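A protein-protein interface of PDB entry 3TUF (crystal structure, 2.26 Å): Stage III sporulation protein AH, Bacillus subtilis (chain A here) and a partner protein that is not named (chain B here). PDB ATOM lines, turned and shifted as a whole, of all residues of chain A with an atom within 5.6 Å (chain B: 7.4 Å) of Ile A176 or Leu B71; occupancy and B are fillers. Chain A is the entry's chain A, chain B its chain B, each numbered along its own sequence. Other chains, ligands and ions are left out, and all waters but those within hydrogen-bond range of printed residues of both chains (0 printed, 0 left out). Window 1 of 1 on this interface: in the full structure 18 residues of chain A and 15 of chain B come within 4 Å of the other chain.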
ATOM      1  N   LYS A 169      -3.966   4.987 -10.448  1.00  0.00           N
ATOM      2  CA  LYS A 169      -4.462   4.297  -9.259  1.00  0.00           C
ATOM      3  C   LYS A 169      -3.481   4.436  -8.076  1.00  0.00           C
ATOM      4  O   LYS A 169      -3.904   4.608  -6.908  1.00  0.00           O
ATOM      5  CB  LYS A 169      -4.661   2.832  -9.575  1.00  0.00           C
ATOM      6  CG  LYS A 169      -5.692   2.539 -10.629  1.00  0.00           C
ATOM      7  CD  LYS A 169      -6.605   1.403 -10.123  1.00  0.00           C
ATOM      8  CE  LYS A 169      -7.562   0.836 -11.186  1.00  0.00           C
ATOM      9  NZ  LYS A 169      -7.069  -0.514 -11.566  1.00  0.00           N
ATOM     10  N   LYS A 171      -1.355   7.075  -7.578  1.00  0.00           N
ATOM     11  CA  LYS A 171      -1.451   8.454  -7.095  1.00  0.00           C
ATOM     12  C   LYS A 171      -2.689   8.711  -6.265  1.00  0.00           C
ATOM     13  O   LYS A 171      -2.641   9.454  -5.273  1.00  0.00           O
ATOM     14  CB  LYS A 171      -1.392   9.424  -8.251  1.00  0.00           C
ATOM     15  CG  LYS A 171      -0.027   9.386  -8.919  1.00  0.00           C
ATOM     16  CD  LYS A 171       0.337  10.736  -9.567  1.00  0.00           C
ATOM     17  CE  LYS A 171       1.658  10.637 -10.349  1.00  0.00           C
ATOM     18  NZ  LYS A 171       2.502  11.893 -10.349  1.00  0.00           N
ATOM     19  N   ALA A 172      -3.779   8.056  -6.634  1.00  0.00           N
ATOM     20  CA  ALA A 172      -5.074   8.326  -6.017  1.00  0.00           C
ATOM     21  C   ALA A 172      -5.147   7.691  -4.677  1.00  0.00           C
ATOM     22  O   ALA A 172      -5.759   8.196  -3.726  1.00  0.00           O
ATOM     23  CB  ALA A 172      -6.101   7.769  -6.824  1.00  0.00           C
ATOM     24  N   THR A 173      -4.531   6.526  -4.620  1.00  0.00           N
ATOM     25  CA  THR A 173      -4.572   5.761  -3.392  1.00  0.00           C
ATOM     26  C   THR A 173      -3.641   6.445  -2.328  1.00  0.00           C
ATOM     27  O   THR A 173      -3.947   6.512  -1.091  1.00  0.00           O
ATOM     28  CB  THR A 173      -4.296   4.316  -3.736  1.00  0.00           C
ATOM     29  OG1 THR A 173      -4.845   3.477  -2.713  1.00  0.00           O
ATOM     30  CG2 THR A 173      -2.807   4.081  -3.923  1.00  0.00           C
ATOM     31  N   ALA A 174      -2.538   7.014  -2.788  1.00  0.00           N
ATOM     32  CA  ALA A 174      -1.695   7.776  -1.849  1.00  0.00           C
ATOM     33  C   ALA A 174      -2.464   9.017  -1.313  1.00  0.00           C
ATOM     34  O   ALA A 174      -2.347   9.361  -0.130  1.00  0.00           O
ATOM     35  CB  ALA A 174      -0.374   8.157  -2.491  1.00  0.00           C
ATOM     36  N   ILE A 175      -3.288   9.645  -2.145  1.00  0.00           N
ATOM     37  CA  ILE A 175      -4.141  10.706  -1.618  1.00  0.00           C
ATOM     38  C   ILE A 175      -5.197  10.190  -0.651  1.00  0.00           C
ATOM     39  O   ILE A 175      -5.368  10.713   0.436  1.00  0.00           O
ATOM     40  CB  ILE A 175      -4.752  11.467  -2.731  1.00  0.00           C
ATOM     41  CG1 ILE A 175      -3.621  12.266  -3.416  1.00  0.00           C
ATOM     42  CG2 ILE A 175      -5.991  12.350  -2.222  1.00  0.00           C
ATOM     43  CD1 ILE A 175      -4.123  13.088  -4.606  1.00  0.00           C
ATOM     44  N   ILE A 176      -5.893   9.127  -1.018  1.00  0.00           N
ATOM     45  CA  ILE A 176      -6.930   8.575  -0.135  1.00  0.00           C
ATOM     46  C   ILE A 176      -6.321   8.114   1.175  1.00  0.00           C
ATOM     47  O   ILE A 176      -6.970   8.120   2.224  1.00  0.00           O
ATOM     48  CB  ILE A 176      -7.740   7.437  -0.811  1.00  0.00           C
ATOM     49  CG1 ILE A 176      -8.601   8.002  -1.912  1.00  0.00           C
ATOM     50  CG2 ILE A 176      -8.640   6.716   0.218  1.00  0.00           C
ATOM     51  CD1 ILE A 176      -9.128   6.862  -2.855  1.00  0.00           C
ATOM     52  N   ASP A 177      -5.047   7.745   1.129  1.00  0.00           N
ATOM     53  CA  ASP A 177      -4.381   7.362   2.416  1.00  0.00           C
ATOM     54  C   ASP A 177      -4.318   8.501   3.455  1.00  0.00           C
ATOM     55  O   ASP A 177      -4.424   8.230   4.675  1.00  0.00           O
ATOM     56  CB  ASP A 177      -3.048   6.653   2.178  1.00  0.00           C
ATOM     57  CG  ASP A 177      -3.251   5.268   1.551  1.00  0.00           C
ATOM     58  OD1 ASP A 177      -4.435   4.738   1.627  1.00  0.00           O
ATOM     59  OD2 ASP A 177      -2.246   4.737   0.981  1.00  0.00           O
ATOM     60  N   LEU A 178      -4.246   9.764   2.965  1.00  0.00           N
ATOM     61  CA  LEU A 178      -4.260  10.954   3.875  1.00  0.00           C
ATOM     62  C   LEU A 178      -5.578  11.139   4.661  1.00  0.00           C
ATOM     63  O   LEU A 178      -5.606  11.843   5.679  1.00  0.00           O
ATOM     64  CB  LEU A 178      -3.839  12.207   3.160  1.00  0.00           C
ATOM     65  CG  LEU A 178      -2.595  11.971   2.319  1.00  0.00           C
ATOM     66  CD1 LEU A 178      -2.384  13.185   1.367  1.00  0.00           C
ATOM     67  CD2 LEU A 178      -1.372  11.713   3.166  1.00  0.00           C
ATOM     68  N   VAL A 179      -6.654  10.507   4.204  1.00  0.00           N
ATOM     69  CA  VAL A 179      -7.976  10.758   4.824  1.00  0.00           C
ATOM     70  C   VAL A 179      -8.120   9.907   6.032  1.00  0.00           C
ATOM     71  O   VAL A 179      -7.676   8.765   6.022  1.00  0.00           O
ATOM     72  CB  VAL A 179      -9.134  10.420   3.833  1.00  0.00           C
ATOM     73  CG1 VAL A 179     -10.522  10.602   4.516  1.00  0.00           C
ATOM     74  CG2 VAL A 179      -9.005  11.282   2.629  1.00  0.00           C
ATOM     75  N   LYS A 184     -13.271   7.364   5.883  1.00  0.00           N
ATOM     76  CA  LYS A 184     -13.265   6.316   4.888  1.00  0.00           C
ATOM     77  C   LYS A 184     -14.186   5.174   5.286  1.00  0.00           C
ATOM     78  O   LYS A 184     -14.800   4.560   4.435  1.00  0.00           O
ATOM     79  CB  LYS A 184     -11.847   5.820   4.608  1.00  0.00           C
ATOM     80  CG  LYS A 184     -11.078   6.733   3.649  1.00  0.00           C
ATOM     81  CD  LYS A 184      -9.537   6.352   3.573  1.00  0.00           C
ATOM     82  CE  LYS A 184      -8.773   6.445   4.882  1.00  0.00           C
ATOM     83  NZ  LYS A 184      -7.319   6.095   4.686  1.00  0.00           N
ATOM     84  N   VAL A 189     -15.279   8.537  -0.832  1.00  0.00           N
ATOM     85  CA  VAL A 189     -14.227   9.484  -1.014  1.00  0.00           C
ATOM     86  C   VAL A 189     -13.936   9.487  -2.507  1.00  0.00           C
ATOM     87  O   VAL A 189     -13.694   8.450  -3.098  1.00  0.00           O
ATOM     88  CB  VAL A 189     -12.953   8.988  -0.272  1.00  0.00           C
ATOM     89  CG1 VAL A 189     -11.751   9.810  -0.670  1.00  0.00           C
ATOM     90  CG2 VAL A 189     -13.101   9.003   1.262  1.00  0.00           C
ATOM     91  N   VAL A 191     -11.644  11.322  -5.786  1.00  0.00           N
ATOM     92  CA  VAL A 191     -10.470  12.131  -6.017  1.00  0.00           C
ATOM     93  C   VAL A 191     -10.388  12.345  -7.475  1.00  0.00           C
ATOM     94  O   VAL A 191     -10.250  11.364  -8.231  1.00  0.00           O
ATOM     95  CB  VAL A 191      -9.230  11.359  -5.660  1.00  0.00           C
ATOM     96  CG1 VAL A 191      -7.948  12.186  -5.928  1.00  0.00           C
ATOM     97  CG2 VAL A 191      -9.336  10.974  -4.225  1.00  0.00           C
ATOM     98  N   LYS B  55     -14.176  -7.272  -8.139  1.00  0.00           N
ATOM     99  CA  LYS B  55     -13.743  -6.179  -7.325  1.00  0.00           C
ATOM    100  C   LYS B  55     -14.344  -6.267  -5.932  1.00  0.00           C
ATOM    101  O   LYS B  55     -15.537  -6.633  -5.741  1.00  0.00           O
ATOM    102  CB  LYS B  55     -14.049  -4.838  -7.967  1.00  0.00           C
ATOM    103  CG  LYS B  55     -13.447  -3.642  -7.179  1.00  0.00           C
ATOM    104  CD  LYS B  55     -14.181  -2.287  -7.529  1.00  0.00           C
ATOM    105  CE  LYS B  55     -13.986  -1.892  -9.018  1.00  0.00           C
ATOM    106  NZ  LYS B  55     -12.571  -2.171  -9.431  1.00  0.00           N
ATOM    107  N   LYS B  56     -13.468  -5.934  -4.978  1.00  0.00           N
ATOM    108  CA  LYS B  56     -13.715  -6.028  -3.527  1.00  0.00           C
ATOM    109  C   LYS B  56     -14.020  -4.645  -2.945  1.00  0.00           C
ATOM    110  O   LYS B  56     -13.733  -3.614  -3.594  1.00  0.00           O
ATOM    111  CB  LYS B  56     -12.478  -6.616  -2.802  1.00  0.00           C
ATOM    112  CG  LYS B  56     -12.201  -8.061  -3.091  1.00  0.00           C
ATOM    113  CD  LYS B  56     -10.831  -8.440  -2.431  1.00  0.00           C
ATOM    114  CE  LYS B  56     -10.392  -9.844  -2.875  1.00  0.00           C
ATOM    115  NZ  LYS B  56      -9.008 -10.219  -2.417  1.00  0.00           N
ATOM    116  N   PHE B  57     -14.595  -4.661  -1.732  1.00  0.00           N
ATOM    117  CA  PHE B  57     -14.955  -3.498  -0.993  1.00  0.00           C
ATOM    118  C   PHE B  57     -13.621  -2.891  -0.478  1.00  0.00           C
ATOM    119  O   PHE B  57     -12.778  -3.587  -0.002  1.00  0.00           O
ATOM    120  CB  PHE B  57     -15.853  -3.980   0.134  1.00  0.00           C
ATOM    121  CG  PHE B  57     -16.191  -2.927   1.127  1.00  0.00           C
ATOM    122  CD1 PHE B  57     -15.262  -2.518   2.075  1.00  0.00           C
ATOM    123  CD2 PHE B  57     -17.444  -2.336   1.125  1.00  0.00           C
ATOM    124  CE1 PHE B  57     -15.592  -1.492   3.043  1.00  0.00           C
ATOM    125  CE2 PHE B  57     -17.791  -1.316   2.068  1.00  0.00           C
ATOM    126  CZ  PHE B  57     -16.884  -0.889   3.018  1.00  0.00           C
ATOM    127  N   TYR B  58     -13.464  -1.578  -0.592  1.00  0.00           N
ATOM    128  CA  TYR B  58     -12.219  -0.934  -0.176  1.00  0.00           C
ATOM    129  C   TYR B  58     -11.954  -1.067   1.327  1.00  0.00           C
ATOM    130  O   TYR B  58     -12.799  -0.702   2.144  1.00  0.00           O
ATOM    131  CB  TYR B  58     -12.223   0.544  -0.577  1.00  0.00           C
ATOM    132  CG  TYR B  58     -10.880   1.222  -0.432  1.00  0.00           C
ATOM    133  CD1 TYR B  58     -10.526   1.861   0.748  1.00  0.00           C
ATOM    134  CD2 TYR B  58      -9.964   1.223  -1.477  1.00  0.00           C
ATOM    135  CE1 TYR B  58      -9.299   2.482   0.886  1.00  0.00           C
ATOM    136  CE2 TYR B  58      -8.736   1.842  -1.350  1.00  0.00           C
ATOM    137  CZ  TYR B  58      -8.408   2.470  -0.166  1.00  0.00           C
ATOM    138  OH  TYR B  58      -7.186   3.086  -0.034  1.00  0.00           O
ATOM    139  N   THR B  60      -9.129   0.071   4.270  1.00  0.00           N
ATOM    140  CA  THR B  60      -8.023   1.029   4.412  1.00  0.00           C
ATOM    141  C   THR B  60      -6.697   0.396   4.885  1.00  0.00           C
ATOM    142  O   THR B  60      -5.605   0.976   4.674  1.00  0.00           O
ATOM    143  CB  THR B  60      -8.371   2.203   5.393  1.00  0.00           C
ATOM    144  OG1 THR B  60      -7.998   1.811   6.691  1.00  0.00           O
ATOM    145  CG2 THR B  60      -9.866   2.456   5.457  1.00  0.00           C
ATOM    146  N   GLU B  65      -1.539  -2.684  -3.204  1.00  0.00           N
ATOM    147  CA  GLU B  65      -2.099  -3.389  -4.353  1.00  0.00           C
ATOM    148  C   GLU B  65      -3.586  -3.659  -4.242  1.00  0.00           C
ATOM    149  O   GLU B  65      -4.324  -3.464  -5.202  1.00  0.00           O
ATOM    150  CB  GLU B  65      -1.361  -4.715  -4.549  1.00  0.00           C
ATOM    151  CG  GLU B  65      -0.894  -4.940  -5.973  1.00  0.00           C
ATOM    152  CD  GLU B  65       0.120  -3.900  -6.418  1.00  0.00           C
ATOM    153  OE1 GLU B  65       0.016  -2.717  -6.002  1.00  0.00           O
ATOM    154  OE2 GLU B  65       1.030  -4.274  -7.191  1.00  0.00           O
ATOM    155  N   GLU B  66      -4.021  -4.093  -3.072  1.00  0.00           N
ATOM    156  CA  GLU B  66      -5.427  -4.402  -2.862  1.00  0.00           C
ATOM    157  C   GLU B  66      -6.266  -3.167  -2.740  1.00  0.00           C
ATOM    158  O   GLU B  66      -7.433  -3.194  -3.093  1.00  0.00           O
ATOM    159  CB  GLU B  66      -5.600  -5.164  -1.572  1.00  0.00           C
ATOM    160  CG  GLU B  66      -4.578  -6.234  -1.338  1.00  0.00           C
ATOM    161  CD  GLU B  66      -5.244  -7.569  -1.314  1.00  0.00           C
ATOM    162  OE1 GLU B  66      -6.245  -7.737  -2.093  1.00  0.00           O
ATOM    163  OE2 GLU B  66      -4.786  -8.424  -0.493  1.00  0.00           O
ATOM    164  N   LYS B  67      -5.692  -2.099  -2.186  1.00  0.00           N
ATOM    165  CA  LYS B  67      -6.389  -0.802  -2.173  1.00  0.00           C
ATOM    166  C   LYS B  67      -6.536  -0.287  -3.585  1.00  0.00           C
ATOM    167  O   LYS B  67      -7.622   0.152  -3.956  1.00  0.00           O
ATOM    168  CB  LYS B  67      -5.668   0.174  -1.305  1.00  0.00           C
ATOM    169  CG  LYS B  67      -5.930  -0.176   0.112  1.00  0.00           C
ATOM    170  CD  LYS B  67      -5.406   0.958   1.010  1.00  0.00           C
ATOM    171  CE  LYS B  67      -3.875   0.994   1.014  1.00  0.00           C
ATOM    172  NZ  LYS B  67      -3.444   2.023   2.050  1.00  0.00           N
ATOM    173  N   GLU B  68      -5.455  -0.386  -4.370  1.00  0.00           N
ATOM    174  CA  GLU B  68      -5.472   0.070  -5.754  1.00  0.00           C
ATOM    175  C   GLU B  68      -6.536  -0.668  -6.582  1.00  0.00           C
ATOM    176  O   GLU B  68      -7.226  -0.112  -7.453  1.00  0.00           O
ATOM    177  CB  GLU B  68      -4.101  -0.148  -6.377  1.00  0.00           C
ATOM    178  CG  GLU B  68      -3.260   1.099  -6.367  1.00  0.00           C
ATOM    179  CD  GLU B  68      -1.860   0.754  -6.618  1.00  0.00           C
ATOM    180  OE1 GLU B  68      -1.468  -0.278  -6.057  1.00  0.00           O
ATOM    181  OE2 GLU B  68      -1.149   1.449  -7.355  1.00  0.00           O
ATOM    182  N   ALA B  69      -6.678  -1.938  -6.301  1.00  0.00           N
ATOM    183  CA  ALA B  69      -7.582  -2.722  -7.050  1.00  0.00           C
ATOM    184  C   ALA B  69      -8.985  -2.573  -6.486  1.00  0.00           C
ATOM    185  O   ALA B  69      -9.908  -3.021  -7.152  1.00  0.00           O
ATOM    186  CB  ALA B  69      -7.117  -4.204  -7.063  1.00  0.00           C
ATOM    187  N   ALA B  70      -9.189  -1.974  -5.301  1.00  0.00           N
ATOM    188  CA  ALA B  70     -10.589  -1.730  -4.807  1.00  0.00           C
ATOM    189  C   ALA B  70     -11.069  -0.298  -5.129  1.00  0.00           C
ATOM    190  O   ALA B  70     -11.928   0.302  -4.411  1.00  0.00           O
ATOM    191  CB  ALA B  70     -10.751  -2.019  -3.284  1.00  0.00           C
ATOM    192  N   LEU B  71     -10.505   0.264  -6.200  1.00  0.00           N
ATOM    193  CA  LEU B  71     -10.903   1.601  -6.610  1.00  0.00           C
ATOM    194  C   LEU B  71     -11.881   1.551  -7.766  1.00  0.00           C
ATOM    195  O   LEU B  71     -11.713   0.744  -8.709  1.00  0.00           O
ATOM    196  CB  LEU B  71      -9.700   2.461  -6.995  1.00  0.00           C
ATOM    197  CG  LEU B  71      -8.810   2.999  -5.869  1.00  0.00           C
ATOM    198  CD1 LEU B  71      -7.706   3.837  -6.498  1.00  0.00           C
ATOM    199  CD2 LEU B  71      -9.537   3.820  -4.751  1.00  0.00           C
ATOM    200  N   VAL B  72     -12.893   2.404  -7.678  1.00  0.00           N
ATOM    201  CA  VAL B  72     -13.766   2.654  -8.814  1.00  0.00           C
ATOM    202  C   VAL B  72     -13.182   3.776  -9.685  1.00  0.00           C
ATOM    203  O   VAL B  72     -13.039   4.876  -9.205  1.00  0.00           O
ATOM    204  CB  VAL B  72     -15.144   3.066  -8.338  1.00  0.00           C
ATOM    205  CG1 VAL B  72     -15.913   3.683  -9.487  1.00  0.00           C
ATOM    206  CG2 VAL B  72     -15.846   1.844  -7.749  1.00  0.00           C
ATOM    207  N   THR B  73     -12.874   3.475 -10.931  1.00  0.00           N
ATOM    208  CA  THR B  73     -12.367   4.455 -11.856  1.00  0.00           C
ATOM    209  C   THR B  73     -13.388   4.893 -12.884  1.00  0.00           C
ATOM    210  O   THR B  73     -13.898   4.105 -13.651  1.00  0.00           O
ATOM    211  CB  THR B  73     -11.211   3.925 -12.641  1.00  0.00           C
ATOM    212  OG1 THR B  73     -10.316   3.259 -11.770  1.00  0.00           O
ATOM    213  CG2 THR B  73     -10.497   5.034 -13.305  1.00  0.00           C
ATOM    214  N   TYR B  74     -13.646   6.181 -12.899  1.00  0.00           N
ATOM    215  CA  TYR B  74     -14.515   6.788 -13.861  1.00  0.00           C
ATOM    216  C   TYR B  74     -13.810   7.448 -15.025  1.00  0.00           C
ATOM    217  O   TYR B  74     -13.734   6.872 -16.089  1.00  0.00           O
ATOM    218  CB  TYR B  74     -15.384   7.822 -13.180  1.00  0.00           C
ATOM    219  CG  TYR B  74     -16.634   8.191 -13.934  1.00  0.00           C
ATOM    220  CD1 TYR B  74     -16.956   7.589 -15.134  1.00  0.00           C
ATOM    221  CD2 TYR B  74     -17.483   9.165 -13.451  1.00  0.00           C
ATOM    222  CE1 TYR B  74     -18.100   7.942 -15.827  1.00  0.00           C
ATOM    223  CE2 TYR B  74     -18.617   9.520 -14.131  1.00  0.00           C
ATOM    224  CZ  TYR B  74     -18.922   8.909 -15.316  1.00  0.00           C
ATOM    225  OH  TYR B  74     -20.051   9.291 -15.979  1.00  0.00           O
ATOM    226  N   THR B  77     -11.566  10.506 -12.351  1.00  0.00           N
ATOM    227  CA  THR B  77     -12.094  10.392 -11.029  1.00  0.00           C
ATOM    228  C   THR B  77     -11.881   8.958 -10.530  1.00  0.00           C
ATOM    229  O   THR B  77     -12.128   7.982 -11.307  1.00  0.00           O
ATOM    230  CB  THR B  77     -13.529  10.901 -10.998  1.00  0.00           C
ATOM    231  OG1 THR B  77     -13.471  12.330 -10.879  1.00  0.00           O
ATOM    232  CG2 THR B  77     -14.336  10.372  -9.818  1.00  0.00           C
ATOM    233  N   TYR B  78     -11.366   8.832  -9.286  1.00  0.00           N
ATOM    234  CA  TYR B  78     -11.348   7.582  -8.549  1.00  0.00           C
ATOM    235  C   TYR B  78     -12.236   7.644  -7.302  1.00  0.00           C
ATOM    236  O   TYR B  78     -12.308   8.663  -6.615  1.00  0.00           O
ATOM    237  CB  TYR B  78      -9.932   7.322  -8.104  1.00  0.00           C
ATOM    238  CG  TYR B  78      -8.969   7.332  -9.258  1.00  0.00           C
ATOM    239  CD1 TYR B  78      -8.484   6.138  -9.787  1.00  0.00           C
ATOM    240  CD2 TYR B  78      -8.549   8.524  -9.834  1.00  0.00           C
ATOM    241  CE1 TYR B  78      -7.580   6.134 -10.861  1.00  0.00           C
ATOM    242  CE2 TYR B  78      -7.661   8.536 -10.875  1.00  0.00           C
ATOM    243  CZ  TYR B  78      -7.184   7.332 -11.405  1.00  0.00           C
ATOM    244  OH  TYR B  78      -6.290   7.313 -12.475  1.00  0.00           O
ATOM    245  N   SER B  79     -12.905   6.564  -6.976  1.00  0.00           N
ATOM    246  CA  SER B  79     -13.787   6.616  -5.851  1.00  0.00           C
ATOM    247  C   SER B  79     -13.541   5.263  -5.146  1.00  0.00           C
ATOM    248  O   SER B  79     -12.837   4.386  -5.713  1.00  0.00           O
ATOM    249  CB  SER B  79     -15.207   6.870  -6.367  1.00  0.00           C
ATOM    250  OG  SER B  79     -16.197   6.131  -5.667  1.00  0.00           O
ATOM    251  N   LEU B  80     -14.002   5.114  -3.897  1.00  0.00           N
ATOM    252  CA  LEU B  80     -13.685   3.917  -3.091  1.00  0.00           C
ATOM    253  C   LEU B  80     -14.699   2.860  -3.488  1.00  0.00           C
ATOM    254  O   LEU B  80     -15.838   3.225  -3.740  1.00  0.00           O
ATOM    255  CB  LEU B  80     -13.938   4.204  -1.628  1.00  0.00           C
ATOM    256  CG  LEU B  80     -13.049   5.250  -0.918  1.00  0.00           C
ATOM    257  CD1 LEU B  80     -13.331   5.119   0.559  1.00  0.00           C
ATOM    258  CD2 LEU B  80     -11.589   5.078  -1.226  1.00  0.00           C
ATOM    259  N   SER B  81     -14.369   1.555  -3.549  1.00  0.00           N
ATOM    260  CA  SER B  81     -15.462   0.603  -3.867  1.00  0.00           C
ATOM    261  C   SER B  81     -16.356   0.337  -2.625  1.00  0.00           C
ATOM    262  O   SER B  81     -15.824  -0.021  -1.613  1.00  0.00           O
ATOM    263  CB  SER B  81     -14.886  -0.670  -4.393  1.00  0.00           C
ATOM    264  OG  SER B  81     -15.879  -1.674  -4.319  1.00  0.00           O
ATOM    265  N   ASP B  85     -18.043  -6.489  -6.844  1.00  0.00           N
ATOM    266  CA  ASP B  85     -18.476  -6.697  -8.209  1.00  0.00           C
ATOM    267  C   ASP B  85     -18.300  -8.155  -8.563  1.00  0.00           C
ATOM    268  O   ASP B  85     -17.214  -8.716  -8.411  1.00  0.00           O
ATOM    269  CB  ASP B  85     -17.646  -5.868  -9.172  1.00  0.00           C
ATOM    270  CG  ASP B  85     -17.952  -4.338  -9.058  1.00  0.00           C
ATOM    271  OD1 ASP B  85     -18.944  -3.943  -8.333  1.00  0.00           O
ATOM    272  OD2 ASP B  85     -17.198  -3.549  -9.705  1.00  0.00           O
ATOM    273  N   SER B 158     -18.252   1.836 -13.576  1.00  0.00           N
ATOM    274  CA  SER B 158     -17.068   1.022 -13.534  1.00  0.00           C
ATOM    275  C   SER B 158     -16.938   0.241 -14.825  1.00  0.00           C
ATOM    276  O   SER B 158     -17.327  -0.902 -14.881  1.00  0.00           O
ATOM    277  CB  SER B 158     -17.097   0.092 -12.298  1.00  0.00           C
ATOM    278  OG  SER B 158     -18.440  -0.175 -11.870  1.00  0.00           O
ATOM    279  N   ASP B 160     -14.465  -0.934 -16.029  1.00  0.00           N
ATOM    280  CA  ASP B 160     -13.405  -1.926 -15.729  1.00  0.00           C
ATOM    281  C   ASP B 160     -13.885  -3.294 -15.174  1.00  0.00           C
ATOM    282  O   ASP B 160     -13.158  -4.268 -15.250  1.00  0.00           O
ATOM    283  CB  ASP B 160     -12.272  -1.306 -14.838  1.00  0.00           C
ATOM    284  CG  ASP B 160     -12.653  -1.245 -13.338  1.00  0.00           C
ATOM    285  OD1 ASP B 160     -12.280  -2.173 -12.596  1.00  0.00           O
ATOM    286  OD2 ASP B 160     -13.343  -0.283 -12.890  1.00  0.00           O
ATOM    287  N   SER B 161     -15.087  -3.361 -14.613  1.00  0.00           N
ATOM    288  CA  SER B 161     -15.637  -4.592 -14.092  1.00  0.00           C
ATOM    289  C   SER B 161     -16.512  -5.289 -15.154  1.00  0.00           C
ATOM    290  O   SER B 161     -17.407  -6.151 -14.811  1.00  0.00           O
ATOM    291  CB  SER B 161     -16.570  -4.247 -12.948  1.00  0.00           C
ATOM    292  OG  SER B 161     -15.901  -3.550 -11.948  1.00  0.00           O
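Of the 13 printed residues of chain A, 8 touch a printed residue of chain B.
Printed residues of chain A that touch a printed residue of chain B: Lys A169, Ala A172, Thr A173, Ile A176, Asp A177, Lys A184, Val A189 and Val A191.
Among the printed residues, 19 pairs touch across the chains.
Among the printed residues, Asp or Glu carboxylates within 4 Å of a Lys or Arg side-chain nitrogen of the other chain: Asp A177 with Lys B67 (2.9 Å).
The side-chain amino group (NZ) of Lys B67 is in salt-bridge range of the side-chain carboxylate (OD1) of Asp A177 (2.9 Å).
O of Tyr B78 sits at hydrogen-bond distance from N of Val A191 (2.9 Å).
N of Leu B80 sits at hydrogen-bond distance from O of Val A189 (3.4 Å).
NZ of Lys B55 sits at hydrogen-bond distance from O of Leu B71.
O of Ser B81 is in hydrogen-bond range of N of Tyr B58 (3.0 Å).
The backbone NH of Val B72 lies within hydrogen-bond range of the backbone carbonyl oxygen of Ser B79 (2.8 Å).
The backbone carbonyl oxygen (O) of Ile A176 sits at hydrogen-bond distance from the side-chain amino group (NZ) of Lys A184 (3.2 Å).
The backbone carbonyl oxygen (O) of Val A179 lies close to the side-chain amino group (NZ) of Lys A184 (3.0 Å).
Among the printed residues, pairs that only touch across the chains: Lys A169 with Glu B68 (3.1 Å), Val A189 with Ser B79 (3.3 Å), Ile A176 with Leu B80 (3.4 Å), Val A191 with Thr B77 (3.5 Å), Thr A173 with Tyr B58 (3.6 Å), Ile A176 with Leu B71 (3.6 Å), Asp A177 with Tyr B58 (3.6 Å), Thr A173 with Lys B67 (3.7 Å), Lys A169 with Thr B73 (3.7 Å), Val A189 with Tyr B78 (3.8 Å), Ala A172 with Tyr B78 (3.8 Å), Lys A169 with Tyr B78 (3.8 Å), Thr A173 with Glu B68 (3.9 Å), Lys A169 with Leu B71 (3.9 Å), Ile A176 with Tyr B58 (3.9 Å) and Lys A184 with Thr B60 (3.995 Å).
Of the printed residues of chain B, Val A189 touches Tyr B78, Ser B79 and Leu B80.
Printed residues of chain A within 4 Å of Ser B79: Val A189 (3.3 Å).
Printed residues of chain A within 4 Å of Leu B80: Ile A176 and Val A189.
Printed residues of chain B within 4 Å of Thr A173: Tyr B58, Lys B67 and Glu B68.
Printed residues of chain A within 4 Å of Glu B68: Lys A169 (3.1 Å) and Thr A173 (3.9 Å).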
